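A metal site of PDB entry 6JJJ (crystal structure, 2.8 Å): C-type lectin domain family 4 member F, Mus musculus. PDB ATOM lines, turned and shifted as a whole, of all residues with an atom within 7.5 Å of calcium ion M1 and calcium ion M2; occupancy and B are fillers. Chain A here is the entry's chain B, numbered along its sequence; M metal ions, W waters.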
ATOM      1  N   THR A  85      20.957   9.866  -0.959  1.00  0.00           N
ATOM      2  CA  THR A  85      21.954  10.903  -1.202  1.00  0.00           C
ATOM      3  C   THR A  85      22.595  11.315   0.116  1.00  0.00           C
ATOM      4  O   THR A  85      21.940  11.315   1.163  1.00  0.00           O
ATOM      5  CB  THR A  85      21.339  12.126  -1.883  1.00  0.00           C
ATOM      6  OG1 THR A  85      22.312  13.181  -1.954  1.00  0.00           O
ATOM      7  CG2 THR A  85      20.121  12.623  -1.094  1.00  0.00           C
ATOM      8  N   ASP A  86      23.880  11.670   0.050  1.00  0.00           N
ATOM      9  CA  ASP A  86      24.625  12.150   1.205  1.00  0.00           C
ATOM     10  C   ASP A  86      25.119  13.579   1.004  1.00  0.00           C
ATOM     11  O   ASP A  86      26.231  13.935   1.404  1.00  0.00           O
ATOM     12  CB  ASP A  86      25.802  11.229   1.523  1.00  0.00           C
ATOM     13  CG  ASP A  86      26.922  11.288   0.467  1.00  0.00           C
ATOM     14  OD1 ASP A  86      26.742  11.962  -0.570  1.00  0.00           O
ATOM     15  OD2 ASP A  86      27.978  10.662   0.693  1.00  0.00           O
ATOM     16  N   GLN A  87      24.312  14.416   0.372  1.00  0.00           N
ATOM     17  CA  GLN A  87      24.722  15.800   0.156  1.00  0.00           C
ATOM     18  C   GLN A  87      24.935  16.598   1.435  1.00  0.00           C
ATOM     19  O   GLN A  87      26.087  16.823   1.814  1.00  0.00           O
ATOM     20  CB  GLN A  87      23.662  16.544  -0.643  1.00  0.00           C
ATOM     21  CG  GLN A  87      23.977  18.024  -0.838  1.00  0.00           C
ATOM     22  CD  GLN A  87      22.880  18.755  -1.570  1.00  0.00           C
ATOM     23  OE1 GLN A  87      21.929  18.146  -2.066  1.00  0.00           O
ATOM     24  NE2 GLN A  87      22.974  20.066  -1.590  1.00  0.00           N
ATOM     25  N   THR A  89      25.615  16.280   4.523  1.00  0.00           N
ATOM     26  CA  THR A  89      26.961  15.992   5.024  1.00  0.00           C
ATOM     27  C   THR A  89      27.460  14.748   4.297  1.00  0.00           C
ATOM     28  O   THR A  89      26.724  13.774   4.127  1.00  0.00           O
ATOM     29  CB  THR A  89      26.997  15.760   6.537  1.00  0.00           C
ATOM     30  OG1 THR A  89      27.185  14.373   6.809  1.00  0.00           O
ATOM     31  CG2 THR A  89      25.717  16.270   7.177  1.00  0.00           C
ATOM     32  N   GLU A  90      28.727  14.792   3.852  1.00  0.00           N
ATOM     33  CA  GLU A  90      29.256  13.741   2.992  1.00  0.00           C
ATOM     34  C   GLU A  90      29.163  12.364   3.625  1.00  0.00           C
ATOM     35  O   GLU A  90      29.129  11.365   2.894  1.00  0.00           O
ATOM     36  CB  GLU A  90      30.707  14.052   2.642  1.00  0.00           C
ATOM     37  CG  GLU A  90      31.318  13.098   1.656  1.00  0.00           C
ATOM     38  CD  GLU A  90      30.499  12.990   0.380  1.00  0.00           C
ATOM     39  OE1 GLU A  90      29.871  13.997  -0.014  1.00  0.00           O
ATOM     40  OE2 GLU A  90      30.509  11.897  -0.227  1.00  0.00           O
ATOM     41  N   GLY A  91      29.110  12.281   4.949  1.00  0.00           N
ATOM     42  CA  GLY A  91      29.129  10.989   5.610  1.00  0.00           C
ATOM     43  C   GLY A  91      27.788  10.281   5.599  1.00  0.00           C
ATOM     44  O   GLY A  91      27.688   9.150   5.105  1.00  0.00           O
ATOM     45  N   ILE A  92      26.761  10.930   6.139  1.00  0.00           N
ATOM     46  CA  ILE A  92      25.487  10.241   6.320  1.00  0.00           C
ATOM     47  C   ILE A  92      24.722  10.272   5.003  1.00  0.00           C
ATOM     48  O   ILE A  92      24.692  11.285   4.300  1.00  0.00           O
ATOM     49  CB  ILE A  92      24.638  10.864   7.445  1.00  0.00           C
ATOM     50  CG1 ILE A  92      23.864  12.108   6.980  1.00  0.00           C
ATOM     51  CG2 ILE A  92      25.524  11.241   8.630  1.00  0.00           C
ATOM     52  CD1 ILE A  92      24.689  13.243   6.496  1.00  0.00           C
ATOM     53  N   TRP A  93      24.117   9.141   4.641  1.00  0.00           N
ATOM     54  CA  TRP A  93      23.125   9.081   3.588  1.00  0.00           C
ATOM     55  C   TRP A  93      21.743   9.281   4.221  1.00  0.00           C
ATOM     56  O   TRP A  93      21.603   9.254   5.440  1.00  0.00           O
ATOM     57  CB  TRP A  93      23.208   7.753   2.840  1.00  0.00           C
ATOM     58  CG  TRP A  93      24.542   7.484   2.208  1.00  0.00           C
ATOM     59  CD1 TRP A  93      25.607   6.856   2.790  1.00  0.00           C
ATOM     60  CD2 TRP A  93      24.958   7.829   0.884  1.00  0.00           C
ATOM     61  NE1 TRP A  93      26.656   6.782   1.898  1.00  0.00           N
ATOM     62  CE2 TRP A  93      26.278   7.381   0.726  1.00  0.00           C
ATOM     63  CE3 TRP A  93      24.333   8.479  -0.187  1.00  0.00           C
ATOM     64  CZ2 TRP A  93      26.990   7.559  -0.462  1.00  0.00           C
ATOM     65  CZ3 TRP A  93      25.042   8.654  -1.358  1.00  0.00           C
ATOM     66  CH2 TRP A  93      26.355   8.200  -1.483  1.00  0.00           C
ATOM     67  N   ASN A 113      32.843  -2.794  -4.044  1.00  0.00           N
ATOM     68  CA  ASN A 113      33.494  -1.707  -3.302  1.00  0.00           C
ATOM     69  C   ASN A 113      32.736  -0.422  -3.619  1.00  0.00           C
ATOM     70  O   ASN A 113      33.056   0.277  -4.580  1.00  0.00           O
ATOM     71  CB  ASN A 113      34.974  -1.594  -3.671  1.00  0.00           C
ATOM     72  CG  ASN A 113      35.202  -1.510  -5.166  1.00  0.00           C
ATOM     73  OD1 ASN A 113      35.638  -2.464  -5.800  1.00  0.00           O
ATOM     74  ND2 ASN A 113      34.911  -0.347  -5.747  1.00  0.00           N
ATOM     75  N   GLN A 114      31.719  -0.116  -2.804  1.00  0.00           N
ATOM     76  CA  GLN A 114      30.842   1.022  -3.048  1.00  0.00           C
ATOM     77  C   GLN A 114      30.127   1.333  -1.752  1.00  0.00           C
ATOM     78  O   GLN A 114      29.809   0.395  -1.003  1.00  0.00           O
ATOM     79  CB  GLN A 114      29.842   0.697  -4.163  1.00  0.00           C
ATOM     80  CG  GLN A 114      29.403   1.893  -5.004  1.00  0.00           C
ATOM     81  CD  GLN A 114      30.563   2.625  -5.651  1.00  0.00           C
ATOM     82  OE1 GLN A 114      31.129   3.556  -5.058  1.00  0.00           O
ATOM     83  NE2 GLN A 114      30.925   2.229  -6.864  1.00  0.00           N
ATOM     84  N   PRO A 115      29.854   2.611  -1.426  1.00  0.00           N
ATOM     85  CA  PRO A 115      30.157   3.823  -2.206  1.00  0.00           C
ATOM     86  C   PRO A 115      31.637   4.222  -2.222  1.00  0.00           C
ATOM     87  O   PRO A 115      32.357   3.931  -1.269  1.00  0.00           O
ATOM     88  CB  PRO A 115      29.324   4.904  -1.509  1.00  0.00           C
ATOM     89  CG  PRO A 115      29.210   4.417  -0.093  1.00  0.00           C
ATOM     90  CD  PRO A 115      29.151   2.912  -0.172  1.00  0.00           C
ATOM     91  N   ASP A 116      32.060   4.878  -3.301  1.00  0.00           N
ATOM     92  CA  ASP A 116      33.438   5.341  -3.429  1.00  0.00           C
ATOM     93  C   ASP A 116      33.581   6.860  -3.395  1.00  0.00           C
ATOM     94  O   ASP A 116      34.681   7.345  -3.093  1.00  0.00           O
ATOM     95  CB  ASP A 116      34.057   4.820  -4.736  1.00  0.00           C
ATOM     96  CG  ASP A 116      33.242   5.197  -5.958  1.00  0.00           C
ATOM     97  OD1 ASP A 116      32.166   5.796  -5.786  1.00  0.00           O
ATOM     98  OD2 ASP A 116      33.691   4.903  -7.085  1.00  0.00           O
ATOM     99  N   ASN A 117      32.523   7.614  -3.701  1.00  0.00           N
ATOM    100  CA  ASN A 117      32.602   9.070  -3.698  1.00  0.00           C
ATOM    101  C   ASN A 117      33.612   9.566  -4.721  1.00  0.00           C
ATOM    102  O   ASN A 117      34.399  10.490  -4.454  1.00  0.00           O
ATOM    103  CB  ASN A 117      32.954   9.607  -2.305  1.00  0.00           C
ATOM    104  CG  ASN A 117      32.533  11.047  -2.114  1.00  0.00           C
ATOM    105  OD1 ASN A 117      32.111  11.720  -3.065  1.00  0.00           O
ATOM    106  ND2 ASN A 117      32.684  11.553  -0.902  1.00  0.00           N
ATOM    107  N   TRP A 118      33.603   8.958  -5.903  1.00  0.00           N
ATOM    108  CA  TRP A 118      34.623   9.229  -6.906  1.00  0.00           C
ATOM    109  C   TRP A 118      34.614  10.695  -7.329  1.00  0.00           C
ATOM    110  O   TRP A 118      33.575  11.363  -7.357  1.00  0.00           O
ATOM    111  CB  TRP A 118      34.411   8.330  -8.119  1.00  0.00           C
ATOM    112  CG  TRP A 118      35.594   8.257  -9.017  1.00  0.00           C
ATOM    113  CD1 TRP A 118      36.805   7.688  -8.735  1.00  0.00           C
ATOM    114  CD2 TRP A 118      35.693   8.760 -10.356  1.00  0.00           C
ATOM    115  NE1 TRP A 118      37.653   7.814  -9.813  1.00  0.00           N
ATOM    116  CE2 TRP A 118      36.996   8.473 -10.818  1.00  0.00           C
ATOM    117  CE3 TRP A 118      34.811   9.432 -11.202  1.00  0.00           C
ATOM    118  CZ2 TRP A 118      37.427   8.831 -12.093  1.00  0.00           C
ATOM    119  CZ3 TRP A 118      35.248   9.785 -12.465  1.00  0.00           C
ATOM    120  CH2 TRP A 118      36.538   9.488 -12.902  1.00  0.00           C
ATOM    121  N   HIS A 120      34.817  13.252 -10.187  1.00  0.00           N
ATOM    122  CA  HIS A 120      34.543  13.318 -11.608  1.00  0.00           C
ATOM    123  C   HIS A 120      35.324  14.452 -12.269  1.00  0.00           C
ATOM    124  O   HIS A 120      35.862  15.351 -11.604  1.00  0.00           O
ATOM    125  CB  HIS A 120      33.045  13.478 -11.859  1.00  0.00           C
ATOM    126  CG  HIS A 120      32.293  12.184 -11.749  1.00  0.00           C
ATOM    127  ND1 HIS A 120      31.715  11.576 -12.837  1.00  0.00           N
ATOM    128  CD2 HIS A 120      32.037  11.382 -10.685  1.00  0.00           C
ATOM    129  CE1 HIS A 120      31.140  10.450 -12.448  1.00  0.00           C
ATOM    130  NE2 HIS A 120      31.315  10.318 -11.150  1.00  0.00           N
ATOM    131  N   ARG A 125      31.785  15.516  -6.962  1.00  0.00           N
ATOM    132  CA  ARG A 125      31.857  14.288  -6.200  1.00  0.00           C
ATOM    133  C   ARG A 125      30.639  13.426  -6.554  1.00  0.00           C
ATOM    134  O   ARG A 125      29.924  13.702  -7.516  1.00  0.00           O
ATOM    135  CB  ARG A 125      31.958  14.585  -4.707  1.00  0.00           C
ATOM    136  CG  ARG A 125      33.254  15.273  -4.284  1.00  0.00           C
ATOM    137  CD  ARG A 125      34.455  14.381  -4.561  1.00  0.00           C
ATOM    138  NE  ARG A 125      35.661  14.817  -3.849  1.00  0.00           N
ATOM    139  CZ  ARG A 125      36.496  15.747  -4.297  1.00  0.00           C
ATOM    140  NH1 ARG A 125      36.271  16.346  -5.459  1.00  0.00           N
ATOM    141  NH2 ARG A 125      37.566  16.067  -3.581  1.00  0.00           N
ATOM    142  N   GLU A 126      30.396  12.385  -5.772  1.00  0.00           N
ATOM    143  CA  GLU A 126      29.232  11.521  -5.953  1.00  0.00           C
ATOM    144  C   GLU A 126      28.372  11.569  -4.702  1.00  0.00           C
ATOM    145  O   GLU A 126      28.796  11.092  -3.648  1.00  0.00           O
ATOM    146  CB  GLU A 126      29.675  10.090  -6.265  1.00  0.00           C
ATOM    147  CG  GLU A 126      30.449   9.951  -7.558  1.00  0.00           C
ATOM    148  CD  GLU A 126      30.721   8.513  -7.890  1.00  0.00           C
ATOM    149  OE1 GLU A 126      30.925   7.730  -6.939  1.00  0.00           O
ATOM    150  OE2 GLU A 126      30.711   8.155  -9.086  1.00  0.00           O
ATOM    151  N   ASP A 127      27.174  12.149  -4.829  1.00  0.00           N
ATOM    152  CA  ASP A 127      26.238  12.272  -3.712  1.00  0.00           C
ATOM    153  C   ASP A 127      24.836  11.781  -4.068  1.00  0.00           C
ATOM    154  O   ASP A 127      23.874  12.134  -3.388  1.00  0.00           O
ATOM    155  CB  ASP A 127      26.135  13.722  -3.233  1.00  0.00           C
ATOM    156  CG  ASP A 127      27.435  14.247  -2.689  1.00  0.00           C
ATOM    157  OD1 ASP A 127      28.190  13.439  -2.105  1.00  0.00           O
ATOM    158  OD2 ASP A 127      27.707  15.449  -2.854  1.00  0.00           O
ATOM    159  N   CYS A 128      24.701  10.984  -5.126  1.00  0.00           N
ATOM    160  CA  CYS A 128      23.404  10.479  -5.540  1.00  0.00           C
ATOM    161  C   CYS A 128      23.572   9.029  -5.956  1.00  0.00           C
ATOM    162  O   CYS A 128      24.614   8.633  -6.482  1.00  0.00           O
ATOM    163  CB  CYS A 128      22.822  11.332  -6.678  1.00  0.00           C
ATOM    164  SG  CYS A 128      22.302  12.984  -6.139  1.00  0.00           S
ATOM    165  N   HIS A 130      22.163   5.506  -7.879  1.00  0.00           N
ATOM    166  CA  HIS A 130      21.374   4.859  -8.918  1.00  0.00           C
ATOM    167  C   HIS A 130      21.547   3.357  -8.808  1.00  0.00           C
ATOM    168  O   HIS A 130      22.352   2.850  -8.026  1.00  0.00           O
ATOM    169  CB  HIS A 130      21.788   5.359 -10.309  1.00  0.00           C
ATOM    170  CG  HIS A 130      23.222   5.119 -10.644  1.00  0.00           C
ATOM    171  ND1 HIS A 130      23.755   5.387 -11.884  1.00  0.00           N
ATOM    172  CD2 HIS A 130      24.235   4.585  -9.912  1.00  0.00           C
ATOM    173  CE1 HIS A 130      25.036   5.081 -11.886  1.00  0.00           C
ATOM    174  NE2 HIS A 130      25.346   4.573 -10.707  1.00  0.00           N
ATOM    175  N   TRP A 135      23.515  -0.865  -5.884  1.00  0.00           N
ATOM    176  CA  TRP A 135      23.630   0.584  -5.809  1.00  0.00           C
ATOM    177  C   TRP A 135      25.033   1.077  -6.148  1.00  0.00           C
ATOM    178  O   TRP A 135      26.027   0.371  -5.944  1.00  0.00           O
ATOM    179  CB  TRP A 135      23.271   1.084  -4.409  1.00  0.00           C
ATOM    180  CG  TRP A 135      21.919   0.727  -3.979  1.00  0.00           C
ATOM    181  CD1 TRP A 135      20.936   0.166  -4.738  1.00  0.00           C
ATOM    182  CD2 TRP A 135      21.373   0.893  -2.674  1.00  0.00           C
ATOM    183  NE1 TRP A 135      19.808  -0.021  -3.983  1.00  0.00           N
ATOM    184  CE2 TRP A 135      20.053   0.416  -2.716  1.00  0.00           C
ATOM    185  CE3 TRP A 135      21.873   1.407  -1.476  1.00  0.00           C
ATOM    186  CZ2 TRP A 135      19.223   0.434  -1.596  1.00  0.00           C
ATOM    187  CZ3 TRP A 135      21.051   1.423  -0.360  1.00  0.00           C
ATOM    188  CH2 TRP A 135      19.734   0.938  -0.439  1.00  0.00           C
ATOM    189  N   ASN A 136      25.101   2.321  -6.619  1.00  0.00           N
ATOM    190  CA  ASN A 136      26.364   3.020  -6.825  1.00  0.00           C
ATOM    191  C   ASN A 136      26.129   4.515  -6.649  1.00  0.00           C
ATOM    192  O   ASN A 136      25.278   5.084  -7.345  1.00  0.00           O
ATOM    193  CB  ASN A 136      26.961   2.767  -8.219  1.00  0.00           C
ATOM    194  CG  ASN A 136      28.111   3.713  -8.548  1.00  0.00           C
ATOM    195  OD1 ASN A 136      28.951   4.006  -7.689  1.00  0.00           O
ATOM    196  ND2 ASN A 136      28.153   4.195  -9.788  1.00  0.00           N
ATOM    197  N   ASP A 137      26.893   5.151  -5.768  1.00  0.00           N
ATOM    198  CA  ASP A 137      26.794   6.605  -5.641  1.00  0.00           C
ATOM    199  C   ASP A 137      27.393   7.252  -6.888  1.00  0.00           C
ATOM    200  O   ASP A 137      28.352   6.740  -7.483  1.00  0.00           O
ATOM    201  CB  ASP A 137      27.486   7.096  -4.370  1.00  0.00           C
ATOM    202  CG  ASP A 137      28.991   6.934  -4.418  1.00  0.00           C
ATOM    203  OD1 ASP A 137      29.482   6.081  -5.189  1.00  0.00           O
ATOM    204  OD2 ASP A 137      29.676   7.660  -3.663  1.00  0.00           O
ATOM    205  N   MET A 138      26.811   8.373  -7.305  1.00  0.00           N
ATOM    206  CA  MET A 138      27.090   8.944  -8.610  1.00  0.00           C
ATOM    207  C   MET A 138      27.020  10.459  -8.521  1.00  0.00           C
ATOM    208  O   MET A 138      26.427  11.021  -7.585  1.00  0.00           O
ATOM    209  CB  MET A 138      26.110   8.403  -9.665  1.00  0.00           C
ATOM    210  CG  MET A 138      26.322   8.937 -11.063  1.00  0.00           C
ATOM    211  SD  MET A 138      27.949   8.509 -11.703  1.00  0.00           S
ATOM    212  CE  MET A 138      28.015   9.539 -13.168  1.00  0.00           C
ATOM    213  N   ALA A 139      27.637  11.121  -9.491  1.00  0.00           N
ATOM    214  CA  ALA A 139      27.549  12.576  -9.590  1.00  0.00           C
ATOM    215  C   ALA A 139      26.121  12.980  -9.895  1.00  0.00           C
ATOM    216  O   ALA A 139      25.540  12.536 -10.900  1.00  0.00           O
ATOM    217  CB  ALA A 139      28.503  13.097 -10.669  1.00  0.00           C
HETATM  218 CA    CA M   1      28.911  11.047  -1.381  1.00  0.00          CA
HETATM  219 CA    CA M   2      30.610   5.752  -7.707  1.00  0.00          CA
HETATM  220  O   HOH W   1      32.028   3.878  -8.880  1.00  0.00           O
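OD1 of Asn 136 sits close to NE2 of Gln 114.
OE1 of Gln 114 sits close to OD1 of Asp 116 (2.6 Å).
N of Asp 127 sits at hydrogen-bond distance from O of Met 138.
The side-chain carboxylate (OD2) of Asp 137 is in hydrogen-bond range of the backbone NH (N) of Asn 117 (2.8 Å).
The backbone NH of Trp 118 lies close to the side-chain carboxylate of Glu 126.
The side-chain carboxylate (OD1) of Asp 137 lies close to the side-chain amide oxygen (OE1) of Gln 114 (3.0 Å).
OD1 of Asn 117 sits close to OE2 of Glu 90, 3.3 Å away.
The backbone NH of Glu 126 sits at hydrogen-bond distance from the side-chain amide oxygen of Asn 117, 3.3 Å away.
Trp 93 touches calcium ion M1 (CH2 to CA, 3.8 Å).
Asn 117 touches calcium ion M1.
The nearest printed residue that does not touch calcium ion M1 is Asp 137 (4.2 Å).
Gln 114 touches calcium ion M2 (OE1 to CA, 3.5 Å).
Within 4 Å of calcium ion M2: Gln 114, Asp 116, Glu 126, Asn 136 and Asp 137.
The nearest printed residue that does not touch calcium ion M2 is Trp 118 (4.6 Å).
Calcium ion M1 is bound by the side-chain carboxylate (OE2) of Glu 90 (2.1 Å), the backbone carbonyl oxygen (O) of Glu 126 (2.3 Å), the side-chain carboxylate (OD2) of Asp 86 (2.3 Å), the side-chain carboxylate (OD1) of Asp 86 (2.5 Å) and the side-chain carboxylate (OD1) of Asp 127 (2.6 Å).
Calcium ion M2 is bound by the side-chain carboxylate (OE1) of Glu 126 (2.1 Å), the side-chain amide oxygen (OD1) of Asn 136 (2.4 Å), the side-chain carboxylate (OD1) of Asp 116 (2.5 Å), the backbone carbonyl oxygen (O) of Asp 137 (2.5 Å), water W1 (2.6 Å), the side-chain carboxylate (OE2) of Glu 126 (2.8 Å) and the side-chain carboxylate (OD1) of Asp 137 (2.8 Å).
Calcium ion M2 has seven donor atoms within binding distance.
Water W1 lies within hydrogen-bond range of OD2 of Asp 116 (2.7 Å) and NE2 of Gln 114 (2.8 Å).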
